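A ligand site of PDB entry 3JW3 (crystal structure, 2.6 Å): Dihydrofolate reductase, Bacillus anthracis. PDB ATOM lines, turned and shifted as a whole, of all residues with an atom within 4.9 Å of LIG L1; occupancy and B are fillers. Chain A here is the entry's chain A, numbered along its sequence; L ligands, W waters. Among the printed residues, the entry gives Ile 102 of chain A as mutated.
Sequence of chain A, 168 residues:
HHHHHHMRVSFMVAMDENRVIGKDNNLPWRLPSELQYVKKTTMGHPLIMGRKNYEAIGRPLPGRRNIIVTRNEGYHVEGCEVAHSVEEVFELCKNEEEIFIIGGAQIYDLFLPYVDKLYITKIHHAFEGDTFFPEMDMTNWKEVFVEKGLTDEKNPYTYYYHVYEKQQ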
ATOM      1  N   MET A  12      18.873 -26.631   4.860  1.00  0.00           N
ATOM      2  CA  MET A  12      18.764 -27.813   4.013  1.00  0.00           C
ATOM      3  C   MET A  12      19.370 -27.462   2.663  1.00  0.00           C
ATOM      4  O   MET A  12      18.833 -26.626   1.924  1.00  0.00           O
ATOM      5  CB  MET A  12      17.302 -28.208   3.840  1.00  0.00           C
ATOM      6  CG  MET A  12      17.074 -29.326   2.854  1.00  0.00           C
ATOM      7  SD  MET A  12      17.669 -30.905   3.459  1.00  0.00           S
ATOM      8  CE  MET A  12      16.806 -31.091   5.015  1.00  0.00           C
ATOM      9  N   VAL A  13      20.499 -28.081   2.349  1.00  0.00           N
ATOM     10  CA  VAL A  13      21.218 -27.749   1.132  1.00  0.00           C
ATOM     11  C   VAL A  13      21.822 -28.978   0.469  1.00  0.00           C
ATOM     12  O   VAL A  13      22.193 -29.942   1.151  1.00  0.00           O
ATOM     13  CB  VAL A  13      22.282 -26.613   1.393  1.00  0.00           C
ATOM     14  CG1 VAL A  13      23.047 -26.845   2.669  1.00  0.00           C
ATOM     15  CG2 VAL A  13      23.237 -26.445   0.195  1.00  0.00           C
ATOM     16  N   ALA A  14      21.865 -28.947  -0.862  1.00  0.00           N
ATOM     17  CA  ALA A  14      22.651 -29.885  -1.650  1.00  0.00           C
ATOM     18  C   ALA A  14      23.632 -29.093  -2.519  1.00  0.00           C
ATOM     19  O   ALA A  14      23.226 -28.189  -3.240  1.00  0.00           O
ATOM     20  CB  ALA A  14      21.743 -30.749  -2.491  1.00  0.00           C
ATOM     21  N   ILE A  21      25.175 -24.662  -6.142  1.00  0.00           N
ATOM     22  CA  ILE A  21      23.830 -25.057  -5.738  1.00  0.00           C
ATOM     23  C   ILE A  21      22.833 -24.876  -6.879  1.00  0.00           C
ATOM     24  O   ILE A  21      21.761 -25.461  -6.852  1.00  0.00           O
ATOM     25  CB  ILE A  21      23.375 -24.294  -4.454  1.00  0.00           C
ATOM     26  CG1 ILE A  21      23.360 -22.783  -4.691  1.00  0.00           C
ATOM     27  CG2 ILE A  21      24.269 -24.629  -3.286  1.00  0.00           C
ATOM     28  CD1 ILE A  21      22.777 -21.958  -3.543  1.00  0.00           C
ATOM     29  N   GLY A  22      23.206 -24.081  -7.891  1.00  0.00           N
ATOM     30  CA  GLY A  22      22.343 -23.826  -9.043  1.00  0.00           C
ATOM     31  C   GLY A  22      23.041 -23.371 -10.308  1.00  0.00           C
ATOM     32  O   GLY A  22      24.093 -22.729 -10.261  1.00  0.00           O
ATOM     33  N   LYS A  23      22.461 -23.722 -11.454  1.00  0.00           N
ATOM     34  CA  LYS A  23      22.813 -23.149 -12.750  1.00  0.00           C
ATOM     35  C   LYS A  23      21.528 -22.703 -13.453  1.00  0.00           C
ATOM     36  O   LYS A  23      20.604 -23.508 -13.639  1.00  0.00           O
ATOM     37  CB  LYS A  23      23.627 -24.130 -13.611  1.00  0.00           C
ATOM     38  CG  LYS A  23      23.289 -24.111 -15.097  1.00  0.00           C
ATOM     39  CD  LYS A  23      24.405 -24.707 -15.971  1.00  0.00           C
ATOM     40  CE  LYS A  23      25.183 -23.618 -16.748  1.00  0.00           C
ATOM     41  NZ  LYS A  23      25.884 -22.623 -15.858  1.00  0.00           N
ATOM     42  N   ASP A  24      21.463 -21.415 -13.820  1.00  0.00           N
ATOM     43  CA  ASP A  24      20.313 -20.834 -14.554  1.00  0.00           C
ATOM     44  C   ASP A  24      18.983 -21.205 -13.885  1.00  0.00           C
ATOM     45  O   ASP A  24      18.133 -21.846 -14.509  1.00  0.00           O
ATOM     46  CB  ASP A  24      20.329 -21.289 -16.028  1.00  0.00           C
ATOM     47  CG  ASP A  24      21.644 -20.977 -16.741  1.00  0.00           C
ATOM     48  OD1 ASP A  24      22.182 -19.855 -16.587  1.00  0.00           O
ATOM     49  OD2 ASP A  24      22.157 -21.851 -17.484  1.00  0.00           O
ATOM     50  N   ASN A  25      18.827 -20.827 -12.619  1.00  0.00           N
ATOM     51  CA  ASN A  25      17.624 -21.184 -11.830  1.00  0.00           C
ATOM     52  C   ASN A  25      17.205 -22.672 -11.876  1.00  0.00           C
ATOM     53  O   ASN A  25      16.007 -22.996 -11.893  1.00  0.00           O
ATOM     54  CB  ASN A  25      16.444 -20.225 -12.123  1.00  0.00           C
ATOM     55  CG  ASN A  25      16.324 -19.105 -11.085  1.00  0.00           C
ATOM     56  OD1 ASN A  25      17.296 -18.750 -10.398  1.00  0.00           O
ATOM     57  ND2 ASN A  25      15.112 -18.551 -10.947  1.00  0.00           N
ATOM     58  N   ASN A  26      18.195 -23.560 -11.902  1.00  0.00           N
ATOM     59  CA  ASN A  26      17.955 -24.996 -11.952  1.00  0.00           C
ATOM     60  C   ASN A  26      18.983 -25.754 -11.146  1.00  0.00           C
ATOM     61  O   ASN A  26      20.138 -25.364 -11.108  1.00  0.00           O
ATOM     62  CB  ASN A  26      18.053 -25.496 -13.394  1.00  0.00           C
ATOM     63  CG  ASN A  26      16.795 -25.232 -14.194  1.00  0.00           C
ATOM     64  OD1 ASN A  26      15.695 -25.131 -13.638  1.00  0.00           O
ATOM     65  ND2 ASN A  26      16.956 -25.132 -15.519  1.00  0.00           N
ATOM     66  N   LEU A  27      18.555 -26.837 -10.502  1.00  0.00           N
ATOM     67  CA  LEU A  27      19.485 -27.845 -10.011  1.00  0.00           C
ATOM     68  C   LEU A  27      20.290 -28.385 -11.200  1.00  0.00           C
ATOM     69  O   LEU A  27      19.710 -28.876 -12.171  1.00  0.00           O
ATOM     70  CB  LEU A  27      18.718 -28.979  -9.340  1.00  0.00           C
ATOM     71  CG  LEU A  27      18.716 -29.116  -7.817  1.00  0.00           C
ATOM     72  CD1 LEU A  27      18.807 -27.784  -7.086  1.00  0.00           C
ATOM     73  CD2 LEU A  27      17.469 -29.888  -7.405  1.00  0.00           C
ATOM     74  N   TRP A  29      21.771 -31.001 -11.439  1.00  0.00           N
ATOM     75  CA  TRP A  29      21.776 -32.468 -11.369  1.00  0.00           C
ATOM     76  C   TRP A  29      20.355 -32.953 -11.161  1.00  0.00           C
ATOM     77  O   TRP A  29      19.533 -32.216 -10.620  1.00  0.00           O
ATOM     78  CB  TRP A  29      22.643 -32.942 -10.196  1.00  0.00           C
ATOM     79  CG  TRP A  29      22.328 -32.205  -8.890  1.00  0.00           C
ATOM     80  CD1 TRP A  29      21.268 -32.440  -8.062  1.00  0.00           C
ATOM     81  CD2 TRP A  29      23.058 -31.125  -8.302  1.00  0.00           C
ATOM     82  NE1 TRP A  29      21.291 -31.585  -6.992  1.00  0.00           N
ATOM     83  CE2 TRP A  29      22.381 -30.751  -7.113  1.00  0.00           C
ATOM     84  CE3 TRP A  29      24.223 -30.432  -8.656  1.00  0.00           C
ATOM     85  CZ2 TRP A  29      22.834 -29.719  -6.261  1.00  0.00           C
ATOM     86  CZ3 TRP A  29      24.685 -29.385  -7.804  1.00  0.00           C
ATOM     87  CH2 TRP A  29      23.978 -29.053  -6.630  1.00  0.00           C
ATOM     88  N   GLY A  50      13.664 -18.309  -0.841  1.00  0.00           N
ATOM     89  CA  GLY A  50      13.625 -17.034  -1.562  1.00  0.00           C
ATOM     90  C   GLY A  50      12.664 -17.084  -2.729  1.00  0.00           C
ATOM     91  O   GLY A  50      12.341 -18.145  -3.233  1.00  0.00           O
ATOM     92  N   ARG A  51      12.188 -15.916  -3.145  1.00  0.00           N
ATOM     93  CA  ARG A  51      11.254 -15.821  -4.271  1.00  0.00           C
ATOM     94  C   ARG A  51      11.772 -16.555  -5.536  1.00  0.00           C
ATOM     95  O   ARG A  51      11.010 -17.296  -6.177  1.00  0.00           O
ATOM     96  CB  ARG A  51      10.941 -14.363  -4.573  1.00  0.00           C
ATOM     97  CG  ARG A  51       9.796 -14.157  -5.535  1.00  0.00           C
ATOM     98  CD  ARG A  51      10.267 -14.141  -6.983  1.00  0.00           C
ATOM     99  NE  ARG A  51      11.202 -13.053  -7.238  1.00  0.00           N
ATOM    100  CZ  ARG A  51      11.925 -12.922  -8.336  1.00  0.00           C
ATOM    101  NH1 ARG A  51      11.837 -13.830  -9.296  1.00  0.00           N
ATOM    102  NH2 ARG A  51      12.736 -11.898  -8.476  1.00  0.00           N
ATOM    103  N   LYS A  52      13.048 -16.350  -5.868  1.00  0.00           N
ATOM    104  CA  LYS A  52      13.677 -17.000  -7.012  1.00  0.00           C
ATOM    105  C   LYS A  52      13.728 -18.518  -6.851  1.00  0.00           C
ATOM    106  O   LYS A  52      13.426 -19.261  -7.784  1.00  0.00           O
ATOM    107  CB  LYS A  52      15.075 -16.446  -7.254  1.00  0.00           C
ATOM    108  CG  LYS A  52      15.081 -15.046  -7.861  1.00  0.00           C
ATOM    109  CD  LYS A  52      16.480 -14.600  -8.137  1.00  0.00           C
ATOM    110  CE  LYS A  52      16.616 -14.035  -9.530  1.00  0.00           C
ATOM    111  NZ  LYS A  52      18.054 -13.834  -9.871  1.00  0.00           N
ATOM    112  N   ASN A  53      14.085 -18.972  -5.650  1.00  0.00           N
ATOM    113  CA  ASN A  53      14.044 -20.410  -5.358  1.00  0.00           C
ATOM    114  C   ASN A  53      12.631 -20.951  -5.508  1.00  0.00           C
ATOM    115  O   ASN A  53      12.458 -22.027  -6.087  1.00  0.00           O
ATOM    116  CB  ASN A  53      14.584 -20.712  -3.961  1.00  0.00           C
ATOM    117  CG  ASN A  53      14.851 -22.214  -3.744  1.00  0.00           C
ATOM    118  OD1 ASN A  53      15.161 -22.945  -4.694  1.00  0.00           O
ATOM    119  ND2 ASN A  53      14.744 -22.664  -2.500  1.00  0.00           N
ATOM    120  N   ALA A  56      11.499 -21.105  -9.363  1.00  0.00           N
ATOM    121  CA  ALA A  56      12.196 -22.203 -10.011  1.00  0.00           C
ATOM    122  C   ALA A  56      11.635 -23.558  -9.574  1.00  0.00           C
ATOM    123  O   ALA A  56      11.677 -24.509 -10.337  1.00  0.00           O
ATOM    124  CB  ALA A  56      13.685 -22.145  -9.763  1.00  0.00           C
ATOM    125  N   VAL A  69      10.168 -15.667   0.622  1.00  0.00           N
ATOM    126  CA  VAL A  69      10.796 -14.433   1.091  1.00  0.00           C
ATOM    127  C   VAL A  69      11.057 -13.517  -0.101  1.00  0.00           C
ATOM    128  O   VAL A  69      11.698 -13.908  -1.086  1.00  0.00           O
ATOM    129  CB  VAL A  69      12.104 -14.706   1.878  1.00  0.00           C
ATOM    130  CG1 VAL A  69      12.560 -13.435   2.608  1.00  0.00           C
ATOM    131  CG2 VAL A  69      11.909 -15.819   2.867  1.00  0.00           C
ATOM    132  N   THR A  70      10.570 -12.282   0.020  1.00  0.00           N
ATOM    133  CA  THR A  70      10.582 -11.298  -1.059  1.00  0.00           C
ATOM    134  C   THR A  70      10.465  -9.882  -0.493  1.00  0.00           C
ATOM    135  O   THR A  70       9.971  -9.693   0.613  1.00  0.00           O
ATOM    136  CB  THR A  70       9.431 -11.576  -2.058  1.00  0.00           C
ATOM    137  OG1 THR A  70       9.333 -10.495  -2.991  1.00  0.00           O
ATOM    138  CG2 THR A  70       8.093 -11.727  -1.334  1.00  0.00           C
ATOM    139  N   ARG A  71      10.936  -8.897  -1.260  1.00  0.00           N
ATOM    140  CA  ARG A  71      10.779  -7.484  -0.921  1.00  0.00           C
ATOM    141  C   ARG A  71       9.505  -6.919  -1.525  1.00  0.00           C
ATOM    142  O   ARG A  71       9.084  -5.819  -1.207  1.00  0.00           O
ATOM    143  CB  ARG A  71      11.977  -6.687  -1.405  1.00  0.00           C
ATOM    144  CG  ARG A  71      13.282  -7.115  -0.792  1.00  0.00           C
ATOM    145  CD  ARG A  71      14.312  -6.040  -0.989  1.00  0.00           C
ATOM    146  NE  ARG A  71      15.629  -6.438  -0.499  1.00  0.00           N
ATOM    147  CZ  ARG A  71      16.536  -7.094  -1.223  1.00  0.00           C
ATOM    148  NH1 ARG A  71      16.262  -7.459  -2.481  1.00  0.00           N
ATOM    149  NH2 ARG A  71      17.709  -7.399  -0.691  1.00  0.00           N
ATOM    150  N   ASN A  72       8.897  -7.694  -2.413  1.00  0.00           N
ATOM    151  CA  ASN A  72       7.717  -7.283  -3.170  1.00  0.00           C
ATOM    152  C   ASN A  72       6.451  -7.319  -2.303  1.00  0.00           C
ATOM    153  O   ASN A  72       5.877  -8.396  -2.088  1.00  0.00           O
ATOM    154  CB  ASN A  72       7.569  -8.235  -4.374  1.00  0.00           C
ATOM    155  CG  ASN A  72       6.493  -7.815  -5.352  1.00  0.00           C
ATOM    156  OD1 ASN A  72       6.454  -8.307  -6.481  1.00  0.00           O
ATOM    157  ND2 ASN A  72       5.599  -6.921  -4.936  1.00  0.00           N
ATOM    158  N   HIS A  84       8.545 -10.763   4.389  1.00  0.00           N
ATOM    159  CA  HIS A  84       9.352  -9.748   3.711  1.00  0.00           C
ATOM    160  C   HIS A  84      10.673  -9.424   4.428  1.00  0.00           C
ATOM    161  O   HIS A  84      11.417  -8.534   4.022  1.00  0.00           O
ATOM    162  CB  HIS A  84       8.511  -8.501   3.395  1.00  0.00           C
ATOM    163  CG  HIS A  84       7.242  -8.801   2.640  1.00  0.00           C
ATOM    164  ND1 HIS A  84       5.995  -8.733   3.218  1.00  0.00           N
ATOM    165  CD2 HIS A  84       7.032  -9.158   1.354  1.00  0.00           C
ATOM    166  CE1 HIS A  84       5.068  -9.041   2.331  1.00  0.00           C
ATOM    167  NE2 HIS A  84       5.672  -9.304   1.185  1.00  0.00           N
ATOM    168  N   SER A  85      10.961 -10.204   5.463  1.00  0.00           N
ATOM    169  CA  SER A  85      12.158 -10.017   6.259  1.00  0.00           C
ATOM    170  C   SER A  85      12.345 -11.226   7.171  1.00  0.00           C
ATOM    171  O   SER A  85      11.399 -12.008   7.407  1.00  0.00           O
ATOM    172  CB  SER A  85      12.023  -8.747   7.106  1.00  0.00           C
ATOM    173  OG  SER A  85      10.936  -8.886   7.994  1.00  0.00           O
ATOM    174  N   ILE A 102      15.581 -23.521   2.820  1.00  0.00           N
ATOM    175  CA  ILE A 102      15.903 -24.376   1.683  1.00  0.00           C
ATOM    176  C   ILE A 102      16.484 -23.627   0.475  1.00  0.00           C
ATOM    177  O   ILE A 102      16.574 -24.194  -0.609  1.00  0.00           O
ATOM    178  CB  ILE A 102      14.700 -25.295   1.301  1.00  0.00           C
ATOM    179  CG1 ILE A 102      13.491 -24.477   0.864  1.00  0.00           C
ATOM    180  CG2 ILE A 102      14.328 -26.231   2.450  1.00  0.00           C
ATOM    181  CD1 ILE A 102      12.585 -25.230  -0.105  1.00  0.00           C
ATOM    182  N   GLY A 103      16.886 -22.370   0.677  1.00  0.00           N
ATOM    183  CA  GLY A 103      17.549 -21.601  -0.385  1.00  0.00           C
ATOM    184  C   GLY A 103      16.709 -20.528  -1.049  1.00  0.00           C
ATOM    185  O   GLY A 103      15.520 -20.380  -0.736  1.00  0.00           O
ATOM    186  N   GLY A 104      17.298 -19.779  -1.987  1.00  0.00           N
ATOM    187  CA  GLY A 104      18.649 -20.015  -2.486  1.00  0.00           C
ATOM    188  C   GLY A 104      19.758 -19.243  -1.797  1.00  0.00           C
ATOM    189  O   GLY A 104      19.708 -19.017  -0.575  1.00  0.00           O
ATOM    190  N   ALA A 105      20.763 -18.840  -2.576  1.00  0.00           N
ATOM    191  CA  ALA A 105      21.957 -18.204  -2.026  1.00  0.00           C
ATOM    192  C   ALA A 105      21.661 -16.971  -1.177  1.00  0.00           C
ATOM    193  O   ALA A 105      22.164 -16.870  -0.063  1.00  0.00           O
ATOM    194  CB  ALA A 105      22.957 -17.864  -3.131  1.00  0.00           C
ATOM    195  N   GLN A 106      20.846 -16.053  -1.696  1.00  0.00           N
ATOM    196  CA  GLN A 106      20.551 -14.797  -0.976  1.00  0.00           C
ATOM    197  C   GLN A 106      19.812 -15.072   0.315  1.00  0.00           C
ATOM    198  O   GLN A 106      20.053 -14.395   1.318  1.00  0.00           O
ATOM    199  CB  GLN A 106      19.704 -13.863  -1.824  1.00  0.00           C
ATOM    200  CG  GLN A 106      20.367 -13.387  -3.098  1.00  0.00           C
ATOM    201  CD  GLN A 106      19.452 -12.447  -3.878  1.00  0.00           C
ATOM    202  OE1 GLN A 106      19.243 -12.631  -5.090  1.00  0.00           O
ATOM    203  NE2 GLN A 106      18.887 -11.459  -3.184  1.00  0.00           N
ATOM    204  N   ILE A 107      18.919 -16.056   0.290  1.00  0.00           N
ATOM    205  CA  ILE A 107      18.157 -16.442   1.478  1.00  0.00           C
ATOM    206  C   ILE A 107      19.032 -17.221   2.471  1.00  0.00           C
ATOM    207  O   ILE A 107      18.837 -17.109   3.686  1.00  0.00           O
ATOM    208  CB  ILE A 107      16.800 -17.139   1.096  1.00  0.00           C
ATOM    209  CG1 ILE A 107      15.652 -16.137   1.201  1.00  0.00           C
ATOM    210  CG2 ILE A 107      16.479 -18.335   1.990  1.00  0.00           C
ATOM    211  CD1 ILE A 107      15.775 -14.887   0.311  1.00  0.00           C
ATOM    212  N   TYR A 108      20.019 -17.959   1.979  1.00  0.00           N
ATOM    213  CA  TYR A 108      21.011 -18.556   2.873  1.00  0.00           C
ATOM    214  C   TYR A 108      21.814 -17.483   3.605  1.00  0.00           C
ATOM    215  O   TYR A 108      21.986 -17.568   4.817  1.00  0.00           O
ATOM    216  CB  TYR A 108      21.937 -19.527   2.149  1.00  0.00           C
ATOM    217  CG  TYR A 108      21.310 -20.839   1.747  1.00  0.00           C
ATOM    218  CD1 TYR A 108      20.605 -21.605   2.665  1.00  0.00           C
ATOM    219  CD2 TYR A 108      21.452 -21.335   0.457  1.00  0.00           C
ATOM    220  CE1 TYR A 108      20.030 -22.813   2.306  1.00  0.00           C
ATOM    221  CE2 TYR A 108      20.894 -22.534   0.087  1.00  0.00           C
ATOM    222  CZ  TYR A 108      20.188 -23.272   1.011  1.00  0.00           C
ATOM    223  OH  TYR A 108      19.636 -24.467   0.626  1.00  0.00           O
ATOM    224  N   LEU A 110      20.974 -14.451   4.265  1.00  0.00           N
ATOM    225  CA  LEU A 110      19.997 -13.853   5.166  1.00  0.00           C
ATOM    226  C   LEU A 110      19.879 -14.537   6.542  1.00  0.00           C
ATOM    227  O   LEU A 110      19.916 -13.878   7.589  1.00  0.00           O
ATOM    228  CB  LEU A 110      18.644 -13.812   4.453  1.00  0.00           C
ATOM    229  CG  LEU A 110      17.793 -12.541   4.430  1.00  0.00           C
ATOM    230  CD1 LEU A 110      18.577 -11.290   4.070  1.00  0.00           C
ATOM    231  CD2 LEU A 110      16.631 -12.710   3.467  1.00  0.00           C
ATOM    232  N   THR A 131      25.342 -20.082  -9.003  1.00  0.00           N
ATOM    233  CA  THR A 131      24.896 -19.794  -7.640  1.00  0.00           C
ATOM    234  C   THR A 131      25.611 -20.778  -6.711  1.00  0.00           C
ATOM    235  O   THR A 131      25.835 -21.934  -7.058  1.00  0.00           O
ATOM    236  CB  THR A 131      23.374 -19.916  -7.553  1.00  0.00           C
ATOM    237  OG1 THR A 131      22.806 -19.100  -8.582  1.00  0.00           O
ATOM    238  CG2 THR A 131      22.841 -19.438  -6.225  1.00  0.00           C
HETATM  239  P1  LIG L   1      16.896 -16.708  -3.802  1.00  0.00           P
HETATM  240  O1  LIG L   1      17.745 -16.407  -2.624  1.00  0.00           O
HETATM  241  O2  LIG L   1      16.234 -18.025  -3.711  1.00  0.00           O
HETATM  242  O3  LIG L   1      15.797 -15.591  -4.036  1.00  0.00           O
HETATM  243  C1  LIG L   1      16.211 -14.250  -4.168  1.00  0.00           C
HETATM  244  C2  LIG L   1      15.002 -13.398  -3.847  1.00  0.00           C
HETATM  245  O4  LIG L   1      14.741 -13.379  -2.456  1.00  0.00           O
HETATM  246  C3  LIG L   1      15.184 -11.942  -4.236  1.00  0.00           C
HETATM  247  O5  LIG L   1      14.926 -11.739  -5.606  1.00  0.00           O
HETATM  248  C4  LIG L   1      14.146 -11.286  -3.355  1.00  0.00           C
HETATM  249  O6  LIG L   1      12.882 -11.533  -3.925  1.00  0.00           O
HETATM  250  C5  LIG L   1      14.191 -12.120  -2.095  1.00  0.00           C
HETATM  251  N1  LIG L   1      15.069 -11.473  -1.108  1.00  0.00           N
HETATM  252  C6  LIG L   1      16.443 -11.500  -1.090  1.00  0.00           C
HETATM  253  N2  LIG L   1      16.879 -10.801  -0.034  1.00  0.00           N
HETATM  254  C7  LIG L   1      15.800 -10.323   0.634  1.00  0.00           C
HETATM  255  C8  LIG L   1      15.682  -9.539   1.776  1.00  0.00           C
HETATM  256  N3  LIG L   1      16.783  -9.153   2.408  1.00  0.00           N
HETATM  257  N4  LIG L   1      14.437  -9.171   2.251  1.00  0.00           N
HETATM  258  C9  LIG L   1      13.310  -9.607   1.572  1.00  0.00           C
HETATM  259  N5  LIG L   1      13.436 -10.383   0.422  1.00  0.00           N
HETATM  260  C10 LIG L   1      14.662 -10.733  -0.038  1.00  0.00           C
HETATM  261  O7  LIG L   1      17.731 -16.537  -5.170  1.00  0.00           O
HETATM  262  P2  LIG L   1      19.143 -17.052  -5.739  1.00  0.00           P
HETATM  263  O8  LIG L   1      19.108 -16.840  -7.211  1.00  0.00           O
HETATM  264  O9  LIG L   1      20.215 -16.444  -4.914  1.00  0.00           O
HETATM  265  O10 LIG L   1      19.075 -18.629  -5.441  1.00  0.00           O
HETATM  266  C11 LIG L   1      18.230 -19.452  -6.209  1.00  0.00           C
HETATM  267  C12 LIG L   1      19.065 -20.370  -7.094  1.00  0.00           C
HETATM  268  O11 LIG L   1      19.726 -21.363  -6.323  1.00  0.00           O
HETATM  269  C13 LIG L   1      18.227 -21.114  -8.129  1.00  0.00           C
HETATM  270  O12 LIG L   1      18.984 -21.212  -9.304  1.00  0.00           O
HETATM  271  C14 LIG L   1      18.031 -22.494  -7.532  1.00  0.00           C
HETATM  272  O13 LIG L   1      17.966 -23.467  -8.561  1.00  0.00           O
HETATM  273  C15 LIG L   1      19.254 -22.670  -6.628  1.00  0.00           C
HETATM  274  N6  LIG L   1      18.994 -23.393  -5.351  1.00  0.00           N
HETATM  275  C16 LIG L   1      19.612 -24.603  -5.100  1.00  0.00           C
HETATM  276  C17 LIG L   1      19.406 -25.317  -3.900  1.00  0.00           C
HETATM  277  C18 LIG L   1      20.384 -26.393  -3.454  1.00  0.00           C
HETATM  278  O14 LIG L   1      20.726 -26.485  -2.078  1.00  0.00           O
HETATM  279  N7  LIG L   1      20.900 -27.238  -4.355  1.00  0.00           N
HETATM  280  C19 LIG L   1      18.564 -24.747  -2.963  1.00  0.00           C
HETATM  281  C20 LIG L   1      17.944 -23.529  -3.219  1.00  0.00           C
HETATM  282  C21 LIG L   1      18.164 -22.845  -4.413  1.00  0.00           C
HETATM  283  P3  LIG L   1      12.155 -10.467  -4.874  1.00  0.00           P
HETATM  284  O15 LIG L   1      11.956  -9.225  -4.046  1.00  0.00           O
HETATM  285  O16 LIG L   1      13.037 -10.127  -6.047  1.00  0.00           O
HETATM  286  O17 LIG L   1      10.849 -11.057  -5.353  1.00  0.00           O
HETATM  287  C1  LG2 L   2      17.325 -29.613  -2.757  1.00  0.00           C
HETATM  288  N1  LG2 L   2      18.033 -30.486  -2.006  1.00  0.00           N
HETATM  289  C2  LG2 L   2      18.562 -30.139  -0.811  1.00  0.00           C
HETATM  290  N2  LG2 L   2      19.272 -31.045  -0.111  1.00  0.00           N
HETATM  291  N3  LG2 L   2      18.395 -28.887  -0.306  1.00  0.00           N
HETATM  292  C3  LG2 L   2      17.687 -27.955  -0.988  1.00  0.00           C
HETATM  293  N4  LG2 L   2      17.518 -26.709  -0.491  1.00  0.00           N
HETATM  294  C4  LG2 L   2      17.099 -28.303  -2.309  1.00  0.00           C
HETATM  295  C5  LG2 L   2      16.298 -27.264  -3.090  1.00  0.00           C
HETATM  296  C6  LG2 L   2      15.124 -27.908  -3.786  1.00  0.00           C
HETATM  297  C7  LG2 L   2      14.272 -28.715  -3.039  1.00  0.00           C
HETATM  298  C8  LG2 L   2      13.178 -29.364  -3.608  1.00  0.00           C
HETATM  299  O1  LG2 L   2      12.386 -30.148  -2.812  1.00  0.00           O
HETATM  300  C9  LG2 L   2      11.586 -29.574  -1.773  1.00  0.00           C
HETATM  301  C10 LG2 L   2      12.909 -29.186  -5.083  1.00  0.00           C
HETATM  302  O2  LG2 L   2      11.798 -29.811  -5.628  1.00  0.00           O
HETATM  303  C11 LG2 L   2      11.710 -30.363  -6.955  1.00  0.00           C
HETATM  304  C12 LG2 L   2      13.838 -28.283  -5.861  1.00  0.00           C
HETATM  305  O3  LG2 L   2      13.652 -28.056  -7.221  1.00  0.00           O
HETATM  306  C13 LG2 L   2      14.313 -26.972  -7.927  1.00  0.00           C
HETATM  307  C14 LG2 L   2      14.914 -27.687  -5.165  1.00  0.00           C
HETATM  308  O   HOH W   1      14.201  -7.803  -4.235  1.00  0.00           O
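The side-chain hydroxyl of Thr 70 is in hydrogen-bond range of an oxygen (O17) of LIG L1 (2.9 Å).
N of Val 13 lies close to N3 of LG2 L2 (3.5 Å).
A nitrogen (N5) of LIG L1 lies close to the backbone NH of Thr 70, 3.5 Å away.
The backbone NH (N) of Gln 106 sits at hydrogen-bond distance from an oxygen (O1) of LIG L1, 3.3 Å away.
N of Asn 26 is in hydrogen-bond range of O13 of LIG L1, 3.4 Å away.
N of Arg 71 lies within hydrogen-bond range of O15 of LIG L1 (3.0 Å).
N4 of LG2 L2 sits at hydrogen-bond distance from O of Met 12 (2.8 Å).
The backbone NH (N) of Gly 104 sits at hydrogen-bond distance from an oxygen (O2) of LIG L1, 2.7 Å away.
N of Ala 105 lies within hydrogen-bond range of O10 of LIG L1 (3.3 Å).
The guanidinium group (NE) of Arg 51 lies within salt-bridge range of an oxygen (O17) of LIG L1.
O14 of LIG L1 is in hydrogen-bond range of N of Ala 14, at 3.0 Å.
N4 of LG2 L2 lies within hydrogen-bond range of O of Ile 102 (2.7 Å).
The backbone NH (N) of Asn 53 lies within hydrogen-bond range of an oxygen (O2) of LIG L1.
O12 of LIG L1 sits close to N of Asn 25 (3.3 Å).
The backbone carbonyl oxygen (O) of Ile 21 lies close to a nitrogen (N7) of LIG L1, at 3.2 Å.
A nitrogen (N2) of LG2 L2 sits close to the backbone carbonyl oxygen (O) of Val 13 (3.4 Å).
A nitrogen (N4) of LG2 L2 lies within hydrogen-bond range of the side-chain hydroxyl of Tyr 108, at 3.3 Å.
O12 of LIG L1 sits close to OD1 of Asn 25 (3.2 Å).
O1 of LIG L1 lies within hydrogen-bond range of N of Ile 107, at 3.2 Å.
O3 of LIG L1 sits at hydrogen-bond distance from N of Lys 52, 3.4 Å away.
A nitrogen (N7) of LIG L1 is in hydrogen-bond range of the backbone carbonyl oxygen (O) of Ala 14 (2.7 Å).
O4 of LIG L1 lies close to O of Val 69.
Val 13 touches LIG L1.
Leu 27 touches LIG L1 (CD1 to N7, 3.5 Å).
CZ2 of Trp 29 touches N7 of LIG L1, at 3.7 Å.
Gly 50 touches LIG L1.
Asn 72 touches LIG L1 (N to O15, 3.8 Å).
O of His 84 touches C9 of LIG L1, at 3.3 Å.
Ile 102 touches LIG L1 (O to C20, 3.0 Å).
Gly 103 touches LIG L1 (CA to C20, 3.5 Å).
Tyr 108 touches LIG L1 (OH to O14, 3.5 Å).
CD1 of Leu 110 touches N3 of LIG L1, 3.2 Å away.
CG2 of Thr 131 touches O11 of LIG L1, 3.7 Å away.
Hydrophobic or aromatic side chains that line LIG L1: Val 13, Ile 21, Leu 27, Trp 29, Val 69, Ala 105, Ile 107 and Leu 110.
The nearest printed residue that does not touch LIG L1 is Gly 22 (4.1 Å).
Water W1 bridges O15 of LIG L1 (2.7 Å) and NH1 of Arg 71 (2.7 Å).
N of Thr 131 sits at hydrogen-bond distance from O of Gly 22.
The backbone carbonyl oxygen (O) of Gly 103 sits at hydrogen-bond distance from the backbone NH (N) of Gly 50 (2.8 Å).
O of Asn 72 sits at hydrogen-bond distance from NE2 of His 84 (3.4 Å).
The backbone NH (N) of Ile 21 lies within hydrogen-bond range of the backbone carbonyl oxygen (O) of Thr 131, at 3.0 Å.
The backbone NH (N) of Gly 103 lies close to the side-chain hydroxyl (OH) of Tyr 108.
The backbone carbonyl oxygen (O) of Val 69 sits at hydrogen-bond distance from the backbone NH (N) of Arg 51, 2.9 Å away.
O of Gly 103 is in hydrogen-bond range of ND2 of Asn 53, 3.0 Å away.
The backbone carbonyl oxygen of Ile 102 lies within hydrogen-bond range of the side-chain amide nitrogen of Asn 53 (3.0 Å).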
